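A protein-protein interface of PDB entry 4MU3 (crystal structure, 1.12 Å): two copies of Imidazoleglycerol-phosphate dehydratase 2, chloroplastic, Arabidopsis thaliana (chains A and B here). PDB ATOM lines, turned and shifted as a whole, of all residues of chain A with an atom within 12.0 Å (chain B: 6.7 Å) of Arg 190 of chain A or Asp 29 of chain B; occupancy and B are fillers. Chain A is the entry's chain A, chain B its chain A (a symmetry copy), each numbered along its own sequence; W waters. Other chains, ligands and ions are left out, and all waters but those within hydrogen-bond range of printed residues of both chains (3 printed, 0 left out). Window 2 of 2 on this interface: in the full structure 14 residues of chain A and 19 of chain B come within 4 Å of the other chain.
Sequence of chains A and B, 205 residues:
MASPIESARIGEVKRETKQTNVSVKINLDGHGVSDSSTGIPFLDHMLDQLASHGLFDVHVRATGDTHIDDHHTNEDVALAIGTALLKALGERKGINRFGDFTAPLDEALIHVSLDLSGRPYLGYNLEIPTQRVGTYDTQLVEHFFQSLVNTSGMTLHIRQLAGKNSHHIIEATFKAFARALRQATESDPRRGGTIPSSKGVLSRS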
ATOM      1  N   ARG A  92      18.567  38.600   4.167  1.00  0.00           N
ATOM      2  CA  ARG A  92      19.187  37.384   4.771  1.00  0.00           C
ATOM      3  C   ARG A  92      18.803  36.085   4.033  1.00  0.00           C
ATOM      4  O   ARG A  92      18.876  34.998   4.585  1.00  0.00           O
ATOM      5  CB  ARG A  92      18.888  37.288   6.270  1.00  0.00           C
ATOM      6  CG  ARG A  92      19.352  38.528   7.033  1.00  0.00           C
ATOM      7  CD  ARG A  92      18.378  39.053   8.079  1.00  0.00           C
ATOM      8  NE  ARG A  92      18.037  38.030   9.047  1.00  0.00           N
ATOM      9  CZ  ARG A  92      17.115  38.158   9.996  1.00  0.00           C
ATOM     10  NH1 ARG A  92      16.408  39.281  10.155  1.00  0.00           N
ATOM     11  NH2 ARG A  92      16.908  37.137  10.809  1.00  0.00           N
ATOM     12  N   LYS A  93      18.412  36.197   2.781  1.00  0.00           N
ATOM     13  CA  LYS A  93      18.024  35.016   2.019  1.00  0.00           C
ATOM     14  C   LYS A  93      19.223  34.226   1.526  1.00  0.00           C
ATOM     15  O   LYS A  93      20.186  34.768   1.012  1.00  0.00           O
ATOM     16  CB  LYS A  93      17.171  35.445   0.831  1.00  0.00           C
ATOM     17  CG  LYS A  93      15.813  35.990   1.258  1.00  0.00           C
ATOM     18  CD  LYS A  93      14.913  36.345   0.087  1.00  0.00           C
ATOM     19  CE  LYS A  93      13.642  37.034   0.560  1.00  0.00           C
ATOM     20  NZ  LYS A  93      12.749  37.352  -0.583  1.00  0.00           N
ATOM     21  N   GLY A  94      19.140  32.921   1.696  1.00  0.00           N
ATOM     22  CA  GLY A  94      20.089  32.012   1.060  1.00  0.00           C
ATOM     23  C   GLY A  94      21.426  31.846   1.755  1.00  0.00           C
ATOM     24  O   GLY A  94      22.316  31.190   1.210  1.00  0.00           O
ATOM     25  N   ILE A  95      21.570  32.388   2.956  1.00  0.00           N
ATOM     26  CA  ILE A  95      22.832  32.363   3.666  1.00  0.00           C
ATOM     27  C   ILE A  95      22.912  31.167   4.612  1.00  0.00           C
ATOM     28  O   ILE A  95      21.919  30.577   5.033  1.00  0.00           O
ATOM     29  CB  ILE A  95      23.127  33.682   4.413  1.00  0.00           C
ATOM     30  CG1 ILE A  95      22.147  33.956   5.551  1.00  0.00           C
ATOM     31  CG2 ILE A  95      23.206  34.858   3.442  1.00  0.00           C
ATOM     32  CD1 ILE A  95      22.530  35.146   6.408  1.00  0.00           C
ATOM     33  N   ASN A  96      24.127  30.845   5.021  1.00  0.00           N
ATOM     34  CA  ASN A  96      24.303  29.758   5.976  1.00  0.00           C
ATOM     35  C   ASN A  96      23.641  30.080   7.326  1.00  0.00           C
ATOM     36  O   ASN A  96      23.138  29.165   7.984  1.00  0.00           O
ATOM     37  CB  ASN A  96      25.783  29.490   6.199  1.00  0.00           C
ATOM     38  CG  ASN A  96      26.451  28.767   5.036  1.00  0.00           C
ATOM     39  OD1 ASN A  96      25.840  27.910   4.417  1.00  0.00           O
ATOM     40  ND2 ASN A  96      27.694  29.127   4.734  1.00  0.00           N
ATOM     41  N   ARG A  97      23.737  31.332   7.756  1.00  0.00           N
ATOM     42  CA  ARG A  97      23.104  31.892   8.955  1.00  0.00           C
ATOM     43  C   ARG A  97      23.885  31.595  10.236  1.00  0.00           C
ATOM     44  O   ARG A  97      24.019  32.463  11.089  1.00  0.00           O
ATOM     45  CB  ARG A  97      21.631  31.507   9.078  1.00  0.00           C
ATOM     46  CG  ARG A  97      20.846  32.658   9.719  1.00  0.00           C
ATOM     47  CD  ARG A  97      19.411  32.268   9.991  1.00  0.00           C
ATOM     48  NE  ARG A  97      19.303  31.557  11.253  1.00  0.00           N
ATOM     49  CZ  ARG A  97      18.229  30.926  11.673  1.00  0.00           C
ATOM     50  NH1 ARG A  97      17.155  30.798  10.913  1.00  0.00           N
ATOM     51  NH2 ARG A  97      18.218  30.385  12.835  1.00  0.00           N
ATOM     52  N   GLN A 183      31.537  32.347   7.694  1.00  0.00           N
ATOM     53  CA  GLN A 183      30.713  31.185   7.423  1.00  0.00           C
ATOM     54  C   GLN A 183      29.210  31.562   7.425  1.00  0.00           C
ATOM     55  O   GLN A 183      28.463  31.224   6.518  1.00  0.00           O
ATOM     56  CB  GLN A 183      31.022  30.103   8.452  1.00  0.00           C
ATOM     57  CG  GLN A 183      30.159  28.871   8.308  1.00  0.00           C
ATOM     58  CD  GLN A 183      30.548  27.724   9.217  1.00  0.00           C
ATOM     59  OE1 GLN A 183      31.129  27.909  10.285  1.00  0.00           O
ATOM     60  NE2 GLN A 183      30.190  26.501   8.780  1.00  0.00           N
ATOM     61  N   ALA A 184      28.764  32.271   8.457  1.00  0.00           N
ATOM     62  CA  ALA A 184      27.355  32.588   8.609  1.00  0.00           C
ATOM     63  C   ALA A 184      26.804  33.456   7.486  1.00  0.00           C
ATOM     64  O   ALA A 184      25.651  33.334   7.083  1.00  0.00           O
ATOM     65  CB  ALA A 184      27.120  33.257   9.952  1.00  0.00           C
ATOM     66  N   THR A 185      27.633  34.386   7.034  1.00  0.00           N
ATOM     67  CA  THR A 185      27.225  35.350   6.014  1.00  0.00           C
ATOM     68  C   THR A 185      27.324  34.796   4.603  1.00  0.00           C
ATOM     69  O   THR A 185      26.714  35.355   3.690  1.00  0.00           O
ATOM     70  CB  THR A 185      28.014  36.664   6.089  1.00  0.00           C
ATOM     71  OG1 THR A 185      29.415  36.438   5.893  1.00  0.00           O
ATOM     72  CG2 THR A 185      27.775  37.371   7.385  1.00  0.00           C
ATOM     73  N   GLU A 186      28.089  33.729   4.373  1.00  0.00           N
ATOM     74  CA  GLU A 186      28.248  33.161   3.040  1.00  0.00           C
ATOM     75  C   GLU A 186      26.980  32.460   2.579  1.00  0.00           C
ATOM     76  O   GLU A 186      26.161  32.018   3.363  1.00  0.00           O
ATOM     77  CB  GLU A 186      29.448  32.210   2.987  1.00  0.00           C
ATOM     78  CG  GLU A 186      30.770  32.969   2.832  1.00  0.00           C
ATOM     79  CD  GLU A 186      32.026  32.130   2.887  1.00  0.00           C
ATOM     80  OE1 GLU A 186      31.960  30.995   3.401  1.00  0.00           O
ATOM     81  OE2 GLU A 186      33.076  32.631   2.420  1.00  0.00           O
ATOM     82  N   SER A 187      26.867  32.348   1.266  1.00  0.00           N
ATOM     83  CA  SER A 187      25.793  31.618   0.637  1.00  0.00           C
ATOM     84  C   SER A 187      25.829  30.153   0.995  1.00  0.00           C
ATOM     85  O   SER A 187      26.873  29.538   0.975  1.00  0.00           O
ATOM     86  CB  SER A 187      25.942  31.724  -0.886  1.00  0.00           C
ATOM     87  OG  SER A 187      25.770  33.062  -1.308  1.00  0.00           O
ATOM     88  N   ASP A 188      24.659  29.598   1.287  1.00  0.00           N
ATOM     89  CA  ASP A 188      24.479  28.170   1.458  1.00  0.00           C
ATOM     90  C   ASP A 188      24.161  27.641   0.064  1.00  0.00           C
ATOM     91  O   ASP A 188      23.168  28.043  -0.510  1.00  0.00           O
ATOM     92  CB  ASP A 188      23.325  27.897   2.422  1.00  0.00           C
ATOM     93  CG  ASP A 188      23.096  26.430   2.704  1.00  0.00           C
ATOM     94  OD1 ASP A 188      23.312  25.632   1.772  1.00  0.00           O
ATOM     95  OD2 ASP A 188      22.692  26.093   3.855  1.00  0.00           O
ATOM     96  N   PRO A 189      24.998  26.730  -0.484  1.00  0.00           N
ATOM     97  CA  PRO A 189      24.795  26.299  -1.867  1.00  0.00           C
ATOM     98  C   PRO A 189      23.483  25.551  -2.107  1.00  0.00           C
ATOM     99  O   PRO A 189      23.086  25.366  -3.260  1.00  0.00           O
ATOM    100  CB  PRO A 189      26.005  25.393  -2.151  1.00  0.00           C
ATOM    101  CG  PRO A 189      26.380  24.873  -0.797  1.00  0.00           C
ATOM    102  CD  PRO A 189      26.126  26.026   0.145  1.00  0.00           C
ATOM    103  N   ARG A 190      22.848  25.073  -1.046  1.00  0.00           N
ATOM    104  CA  ARG A 190      21.560  24.375  -1.157  1.00  0.00           C
ATOM    105  C   ARG A 190      20.346  25.235  -0.781  1.00  0.00           C
ATOM    106  O   ARG A 190      19.227  24.737  -0.798  1.00  0.00           O
ATOM    107  CB  ARG A 190      21.590  23.088  -0.333  1.00  0.00           C
ATOM    108  CG  ARG A 190      22.538  22.041  -0.902  1.00  0.00           C
ATOM    109  CD  ARG A 190      22.665  20.805  -0.029  1.00  0.00           C
ATOM    110  NE  ARG A 190      21.407  20.074   0.069  1.00  0.00           N
ATOM    111  CZ  ARG A 190      21.202  19.089   0.931  1.00  0.00           C
ATOM    112  NH1 ARG A 190      22.172  18.705   1.751  1.00  0.00           N
ATOM    113  NH2 ARG A 190      20.052  18.466   0.964  1.00  0.00           N
ATOM    114  N   ARG A 191      20.562  26.531  -0.523  1.00  0.00           N
ATOM    115  CA  ARG A 191      19.467  27.468  -0.172  1.00  0.00           C
ATOM    116  C   ARG A 191      19.277  28.583  -1.216  1.00  0.00           C
ATOM    117  O   ARG A 191      18.659  29.600  -0.926  1.00  0.00           O
ATOM    118  CB  ARG A 191      19.637  28.095   1.234  1.00  0.00           C
ATOM    119  CG  ARG A 191      19.664  27.069   2.344  1.00  0.00           C
ATOM    120  CD  ARG A 191      19.820  27.684   3.728  1.00  0.00           C
ATOM    121  NE  ARG A 191      19.931  26.659   4.764  1.00  0.00           N
ATOM    122  CZ  ARG A 191      18.911  26.094   5.395  1.00  0.00           C
ATOM    123  NH1 ARG A 191      17.677  26.464   5.106  1.00  0.00           N
ATOM    124  NH2 ARG A 191      19.142  25.146   6.308  1.00  0.00           N
ATOM    125  N   GLY A 192      19.708  28.346  -2.451  1.00  0.00           N
ATOM    126  CA  GLY A 192      19.547  29.324  -3.547  1.00  0.00           C
ATOM    127  C   GLY A 192      18.158  29.316  -4.163  1.00  0.00           C
ATOM    128  O   GLY A 192      17.224  28.733  -3.614  1.00  0.00           O
ATOM    129  N   SER B   7      20.130   9.573  -8.451  1.00  0.00           N
ATOM    130  CA  SER B   7      18.946  10.233  -7.890  1.00  0.00           C
ATOM    131  C   SER B   7      19.041  10.327  -6.376  1.00  0.00           C
ATOM    132  O   SER B   7      19.971   9.831  -5.746  1.00  0.00           O
ATOM    133  CB  SER B   7      17.684   9.485  -8.283  1.00  0.00           C
ATOM    134  OG  SER B   7      17.753   8.149  -7.844  1.00  0.00           O
ATOM    135  N   ALA B   8      18.043  10.974  -5.817  1.00  0.00           N
ATOM    136  CA  ALA B   8      17.986  11.252  -4.397  1.00  0.00           C
ATOM    137  C   ALA B   8      18.008   9.970  -3.543  1.00  0.00           C
ATOM    138  O   ALA B   8      17.400   8.968  -3.888  1.00  0.00           O
ATOM    139  CB  ALA B   8      16.740  12.067  -4.120  1.00  0.00           C
ATOM    140  N   ARG B   9      18.709  10.032  -2.415  1.00  0.00           N
ATOM    141  CA  ARG B   9      18.786   8.906  -1.464  1.00  0.00           C
ATOM    142  C   ARG B   9      17.601   8.949  -0.503  1.00  0.00           C
ATOM    143  O   ARG B   9      17.540   9.810   0.378  1.00  0.00           O
ATOM    144  CB  ARG B   9      20.097   9.011  -0.724  1.00  0.00           C
ATOM    145  CG  ARG B   9      21.313   8.748  -1.580  1.00  0.00           C
ATOM    146  CD  ARG B   9      22.589   9.066  -0.839  1.00  0.00           C
ATOM    147  NE  ARG B   9      22.622  10.500  -0.556  1.00  0.00           N
ATOM    148  CZ  ARG B   9      23.438  11.081   0.304  1.00  0.00           C
ATOM    149  NH1 ARG B   9      24.265  10.360   1.061  1.00  0.00           N
ATOM    150  NH2 ARG B   9      23.385  12.394   0.477  1.00  0.00           N
ATOM    151  N   ILE B  10      16.647   8.046  -0.716  1.00  0.00           N
ATOM    152  CA  ILE B  10      15.406   8.012   0.035  1.00  0.00           C
ATOM    153  C   ILE B  10      15.316   6.693   0.794  1.00  0.00           C
ATOM    154  O   ILE B  10      15.556   5.633   0.224  1.00  0.00           O
ATOM    155  CB  ILE B  10      14.195   8.219  -0.885  1.00  0.00           C
ATOM    156  CG1 ILE B  10      14.238   9.641  -1.476  1.00  0.00           C
ATOM    157  CG2 ILE B  10      12.884   7.994  -0.135  1.00  0.00           C
ATOM    158  CD1 ILE B  10      13.324   9.885  -2.657  1.00  0.00           C
ATOM    159  N   ILE B  26      12.470   9.509   4.463  1.00  0.00           N
ATOM    160  CA  ILE B  26      13.496  10.558   4.556  1.00  0.00           C
ATOM    161  C   ILE B  26      14.280  10.619   3.261  1.00  0.00           C
ATOM    162  O   ILE B  26      14.720   9.591   2.740  1.00  0.00           O
ATOM    163  CB  ILE B  26      14.476  10.361   5.750  1.00  0.00           C
ATOM    164  CG1 ILE B  26      15.403  11.569   5.901  1.00  0.00           C
ATOM    165  CG2 ILE B  26      15.301   9.095   5.585  1.00  0.00           C
ATOM    166  CD1 ILE B  26      16.023  11.683   7.280  1.00  0.00           C
ATOM    167  N   ASN B  27      14.461  11.833   2.759  1.00  0.00           N
ATOM    168  CA  ASN B  27      15.328  12.126   1.605  1.00  0.00           C
ATOM    169  C   ASN B  27      16.563  12.845   2.115  1.00  0.00           C
ATOM    170  O   ASN B  27      16.464  13.959   2.624  1.00  0.00           O
ATOM    171  CB  ASN B  27      14.581  12.982   0.595  1.00  0.00           C
ATOM    172  CG  ASN B  27      15.329  13.173  -0.709  1.00  0.00           C
ATOM    173  OD1 ASN B  27      16.547  12.988  -0.793  1.00  0.00           O
ATOM    174  ND2 ASN B  27      14.600  13.600  -1.717  1.00  0.00           N
ATOM    175  N   LEU B  28      17.721  12.205   1.990  1.00  0.00           N
ATOM    176  CA  LEU B  28      18.986  12.797   2.419  1.00  0.00           C
ATOM    177  C   LEU B  28      19.391  13.987   1.553  1.00  0.00           C
ATOM    178  O   LEU B  28      20.149  14.833   2.029  1.00  0.00           O
ATOM    179  CB  LEU B  28      20.136  11.792   2.436  1.00  0.00           C
ATOM    180  CG  LEU B  28      19.929  10.531   3.246  1.00  0.00           C
ATOM    181  CD1 LEU B  28      21.145   9.642   3.169  1.00  0.00           C
ATOM    182  CD2 LEU B  28      19.517  10.845   4.676  1.00  0.00           C
ATOM    183  N   ASP B  29      18.881  14.031   0.315  1.00  0.00           N
ATOM    184  CA  ASP B  29      19.189  15.052  -0.657  1.00  0.00           C
ATOM    185  C   ASP B  29      18.004  16.004  -0.855  1.00  0.00           C
ATOM    186  O   ASP B  29      17.701  16.434  -1.957  1.00  0.00           O
ATOM    187  CB  ASP B  29      19.621  14.392  -1.956  1.00  0.00           C
ATOM    188  CG  ASP B  29      20.782  13.428  -1.742  1.00  0.00           C
ATOM    189  OD1 ASP B  29      21.845  13.922  -1.339  1.00  0.00           O
ATOM    190  OD2 ASP B  29      20.621  12.182  -1.934  1.00  0.00           O
ATOM    191  N   GLY B  30      17.360  16.363   0.244  1.00  0.00           N
ATOM    192  CA  GLY B  30      16.126  17.097   0.225  1.00  0.00           C
ATOM    193  C   GLY B  30      16.291  18.594   0.151  1.00  0.00           C
ATOM    194  O   GLY B  30      17.361  19.143  -0.134  1.00  0.00           O
ATOM    195  N   HIS B  31      15.156  19.242   0.364  1.00  0.00           N
ATOM    196  CA  HIS B  31      15.040  20.695   0.385  1.00  0.00           C
ATOM    197  C   HIS B  31      14.390  21.197   1.662  1.00  0.00           C
ATOM    198  O   HIS B  31      13.845  22.287   1.693  1.00  0.00           O
ATOM    199  CB  HIS B  31      14.300  21.177  -0.860  1.00  0.00           C
ATOM    200  CG  HIS B  31      15.032  20.852  -2.111  1.00  0.00           C
ATOM    201  ND1 HIS B  31      14.865  19.663  -2.784  1.00  0.00           N
ATOM    202  CD2 HIS B  31      16.008  21.521  -2.762  1.00  0.00           C
ATOM    203  CE1 HIS B  31      15.679  19.633  -3.824  1.00  0.00           C
ATOM    204  NE2 HIS B  31      16.375  20.753  -3.839  1.00  0.00           N
ATOM    205  N   GLY B  32      14.446  20.398   2.723  1.00  0.00           N
ATOM    206  CA  GLY B  32      13.885  20.808   4.005  1.00  0.00           C
ATOM    207  C   GLY B  32      12.373  20.687   4.120  1.00  0.00           C
ATOM    208  O   GLY B  32      11.766  21.376   4.941  1.00  0.00           O
ATOM    209  N   GLY B  54      18.649  20.623   8.518  1.00  0.00           N
ATOM    210  CA  GLY B  54      19.440  19.616   7.832  1.00  0.00           C
ATOM    211  C   GLY B  54      19.265  19.563   6.320  1.00  0.00           C
ATOM    212  O   GLY B  54      20.014  18.863   5.647  1.00  0.00           O
ATOM    213  N   LEU B  55      18.209  20.219   5.832  1.00  0.00           N
ATOM    214  CA  LEU B  55      17.724  20.125   4.439  1.00  0.00           C
ATOM    215  C   LEU B  55      17.336  18.711   4.062  1.00  0.00           C
ATOM    216  O   LEU B  55      17.248  18.364   2.909  1.00  0.00           O
ATOM    217  CB  LEU B  55      18.704  20.756   3.457  1.00  0.00           C
ATOM    218  CG  LEU B  55      18.841  22.268   3.626  1.00  0.00           C
ATOM    219  CD1 LEU B  55      19.752  22.793   2.544  1.00  0.00           C
ATOM    220  CD2 LEU B  55      17.492  22.990   3.653  1.00  0.00           C
ATOM    221  N   PHE B  56      16.997  17.894   5.026  1.00  0.00           N
ATOM    222  CA  PHE B  56      16.334  16.627   4.749  1.00  0.00           C
ATOM    223  C   PHE B  56      14.880  16.869   4.410  1.00  0.00           C
ATOM    224  O   PHE B  56      14.277  17.796   4.932  1.00  0.00           O
ATOM    225  CB  PHE B  56      16.430  15.741   6.002  1.00  0.00           C
ATOM    226  CG  PHE B  56      17.849  15.500   6.419  1.00  0.00           C
ATOM    227  CD1 PHE B  56      18.703  14.825   5.598  1.00  0.00           C
ATOM    228  CD2 PHE B  56      18.370  16.043   7.576  1.00  0.00           C
ATOM    229  CE1 PHE B  56      20.029  14.656   5.920  1.00  0.00           C
ATOM    230  CE2 PHE B  56      19.697  15.892   7.902  1.00  0.00           C
ATOM    231  CZ  PHE B  56      20.519  15.188   7.065  1.00  0.00           C
ATOM    232  N   ASP B  57      14.300  16.027   3.554  1.00  0.00           N
ATOM    233  CA  ASP B  57      12.834  15.953   3.498  1.00  0.00           C
ATOM    234  C   ASP B  57      12.408  14.863   4.478  1.00  0.00           C
ATOM    235  O   ASP B  57      12.921  13.741   4.410  1.00  0.00           O
ATOM    236  CB  ASP B  57      12.300  15.657   2.092  1.00  0.00           C
ATOM    237  CG  ASP B  57      12.681  16.706   1.093  1.00  0.00           C
ATOM    238  OD1 ASP B  57      13.005  17.849   1.474  1.00  0.00           O
ATOM    239  OD2 ASP B  57      12.636  16.360  -0.111  1.00  0.00           O
ATOM    240  N   ALA B  88      18.482   4.805   3.496  1.00  0.00           N
ATOM    241  CA  ALA B  88      18.771   5.893   2.552  1.00  0.00           C
ATOM    242  C   ALA B  88      20.254   5.986   2.245  1.00  0.00           C
ATOM    243  O   ALA B  88      20.648   6.316   1.149  1.00  0.00           O
ATOM    244  CB  ALA B  88      18.267   7.204   3.082  1.00  0.00           C
ATOM    245  N   ARG B 182      23.657  16.652   8.156  1.00  0.00           N
ATOM    246  CA  ARG B 182      23.762  17.151   6.772  1.00  0.00           C
ATOM    247  C   ARG B 182      25.215  17.037   6.299  1.00  0.00           C
ATOM    248  O   ARG B 182      25.496  16.498   5.233  1.00  0.00           O
ATOM    249  CB  ARG B 182      23.267  18.595   6.677  1.00  0.00           C
ATOM    250  CG  ARG B 182      23.583  19.219   5.354  1.00  0.00           C
ATOM    251  CD  ARG B 182      23.051  20.626   5.185  1.00  0.00           C
ATOM    252  NE  ARG B 182      23.612  21.255   4.008  1.00  0.00           N
ATOM    253  CZ  ARG B 182      23.411  22.505   3.634  1.00  0.00           C
ATOM    254  NH1 ARG B 182      22.623  23.301   4.336  1.00  0.00           N
ATOM    255  NH2 ARG B 182      24.010  22.977   2.553  1.00  0.00           N
ATOM    256  N   THR B 185      26.262  13.299   5.719  1.00  0.00           N
ATOM    257  CA  THR B 185      25.567  12.645   4.611  1.00  0.00           C
ATOM    258  C   THR B 185      25.922  13.237   3.258  1.00  0.00           C
ATOM    259  O   THR B 185      25.685  12.592   2.236  1.00  0.00           O
ATOM    260  CB  THR B 185      24.042  12.658   4.776  1.00  0.00           C
ATOM    261  OG1 THR B 185      23.538  13.998   4.832  1.00  0.00           O
ATOM    262  CG2 THR B 185      23.617  11.890   5.987  1.00  0.00           C
ATOM    263  N   GLU B 186      26.461  14.455   3.200  1.00  0.00           N
ATOM    264  CA  GLU B 186      26.802  15.092   1.933  1.00  0.00           C
ATOM    265  C   GLU B 186      28.008  14.432   1.285  1.00  0.00           C
ATOM    266  O   GLU B 186      28.838  13.820   1.932  1.00  0.00           O
ATOM    267  CB  GLU B 186      27.036  16.595   2.120  1.00  0.00           C
ATOM    268  CG  GLU B 186      25.718  17.374   2.168  1.00  0.00           C
ATOM    269  CD  GLU B 186      25.833  18.852   2.467  1.00  0.00           C
ATOM    270  OE1 GLU B 186      26.881  19.270   3.000  1.00  0.00           O
ATOM    271  OE2 GLU B 186      24.856  19.579   2.171  1.00  0.00           O
ATOM    272  N   SER B 187      28.088  14.608  -0.023  1.00  0.00           N
ATOM    273  CA  SER B 187      29.215  14.156  -0.802  1.00  0.00           C
ATOM    274  C   SER B 187      30.490  14.849  -0.394  1.00  0.00           C
ATOM    275  O   SER B 187      30.511  16.048  -0.213  1.00  0.00           O
ATOM    276  CB  SER B 187      28.964  14.484  -2.279  1.00  0.00           C
ATOM    277  OG  SER B 187      27.862  13.747  -2.770  1.00  0.00           O
HETATM  278  O   HOH W   1      19.210  20.568  -1.743  1.00  0.00           O
HETATM  279  O   HOH W   2      20.589  17.154   3.587  1.00  0.00           O
HETATM  280  O   HOH W   3      21.578  23.642   6.921  1.00  0.00           O
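Ser 187 of chain A touches none of the printed residues of chain B. Of the printed residues of chain B, Asp 188 of chain A touches Arg 182 (2.8 Å). Of chain B, only Leu 28 (3.8 Å), Asp 29 (3.7 Å), Gly 30 (3.0 Å), Leu 55 (3.4 Å), Arg 182 (3.6 Å) and Glu 186 (2.9 Å) come within 4 Å of Arg 190 of chain A. Of the printed residues of chain B, Arg 191 of chain A touches Leu 55. No residue of chain A comes within 4 Å of Ser 7 of chain B. No residue of chain A comes within 4 Å of Arg 9 of chain B. Ile 26 of chain B touches none of the printed residues of chain A. Leu 28 of chain B touches one residue of chain A. Asp 29 of chain B touches just one residue of chain A: Arg 190 (3.7 Å). Gly 30 of chain B touches just one residue of chain A: Arg 190. His 31 of chain B touches none of the printed residues of chain A. No residue of chain A comes within 4 Å of Gly 54 of chain B. No residue of chain A comes within 4 Å of Phe 56 of chain B. Of the printed residues of chain A, Arg 182 of chain B touches Asp 188 and Arg 190. Glu 186 of chain B touches just one residue of chain A: Arg 190. The nearest residue of chain A that does not touch Asp 29 of chain B is Pro 189 of chain A (10.5 Å). The nearest printed residue of chain B that does not touch Asp 188 of chain A is Leu 55 of chain B (4.6 Å).
3 positions are printed for both chains. Of the 8 pairs that touch across the chains among the printed residues, none has its exchanged pair printed and touching as well.
Water W2 lies within hydrogen-bond range of the backbone carbonyl oxygen of Gly 54 of chain B, the backbone carbonyl oxygen of Leu 28 of chain B and the guanidinium group of Arg 190 of chain A. Water W3 bridges the guanidinium group (NH1) of Arg 182 of chain B (2.8 Å) and the guanidinium group (NH2) of Arg 191 of chain A (2.9 Å). Water W1 lies within hydrogen-bond range of O of Gly 30 of chain B and NE of Arg 190 of chain A.
OD2 of Asp 188 of chain A lies within salt-bridge range of NH1 of Arg 182 of chain B, at 2.8 Å. The guanidinium group of Arg 190 of chain A lies within hydrogen-bond range of the backbone carbonyl oxygen of Leu 55 of chain B, at 3.4 Å. O of Gly 30 of chain B sits at hydrogen-bond distance from NH2 of Arg 190 of chain A, at 3.0 Å. OE2 of Glu 186 of chain B lies within salt-bridge range of NH1 of Arg 190 of chain A (2.9 Å).
The backbone carbonyl oxygen of Leu 55 of chain B is in hydrogen-bond range of the backbone NH of His 31 of chain B, at 3.4 Å. The guanidinium group of Arg 182 of chain B lies within salt-bridge range of the side-chain carboxylate of Glu 186 of chain B (2.8 Å). The backbone carbonyl oxygen (O) of Leu 55 of chain B lies close to the backbone NH (N) of Gly 30 of chain B (3.3 Å). The backbone carbonyl oxygen (O) of Arg 182 of chain B is in hydrogen-bond range of the side-chain hydroxyl (OG1) of Thr 185 of chain B. The backbone NH (N) of Asp 29 of chain B is in hydrogen-bond range of the side-chain amide oxygen (OD1) of Asn 27 of chain B (2.8 Å). O of Gly 94 of chain A lies within hydrogen-bond range of N of Asp 188 of chain A (2.8 Å).
O of Leu 28 of chain B touches NH2 of Arg 190 of chain A (3.8 Å). NH2 of Arg 190 of chain A touches C of Asp 29 of chain B (3.7 Å). Arg 182 of chain B touches Arg 190 of chain A (NH2 to CD, 3.6 Å). Leu 55 of chain B touches Arg 191 of chain A (CD2 to NH1, 3.8 Å).
Printed residues of chain B that touch a printed residue of chain A: Leu 28, Asp 29, Gly 30, Leu 55, Arg 182 and Glu 186. Hydrophobic or aromatic side chains of chain B that line the printed part of chain A: Leu 55. Of the 16 printed residues of chain A, 3 touch a printed residue of chain B. Among the printed residues, 8 pairs touch across the chains. Among the printed residues, Asp or Glu carboxylates within 4 Å of a Lys or Arg side-chain nitrogen of the other chain: Asp 188 of chain A with Arg 182 of chain B and Arg 190 of chain A with Glu 186 of chain B.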
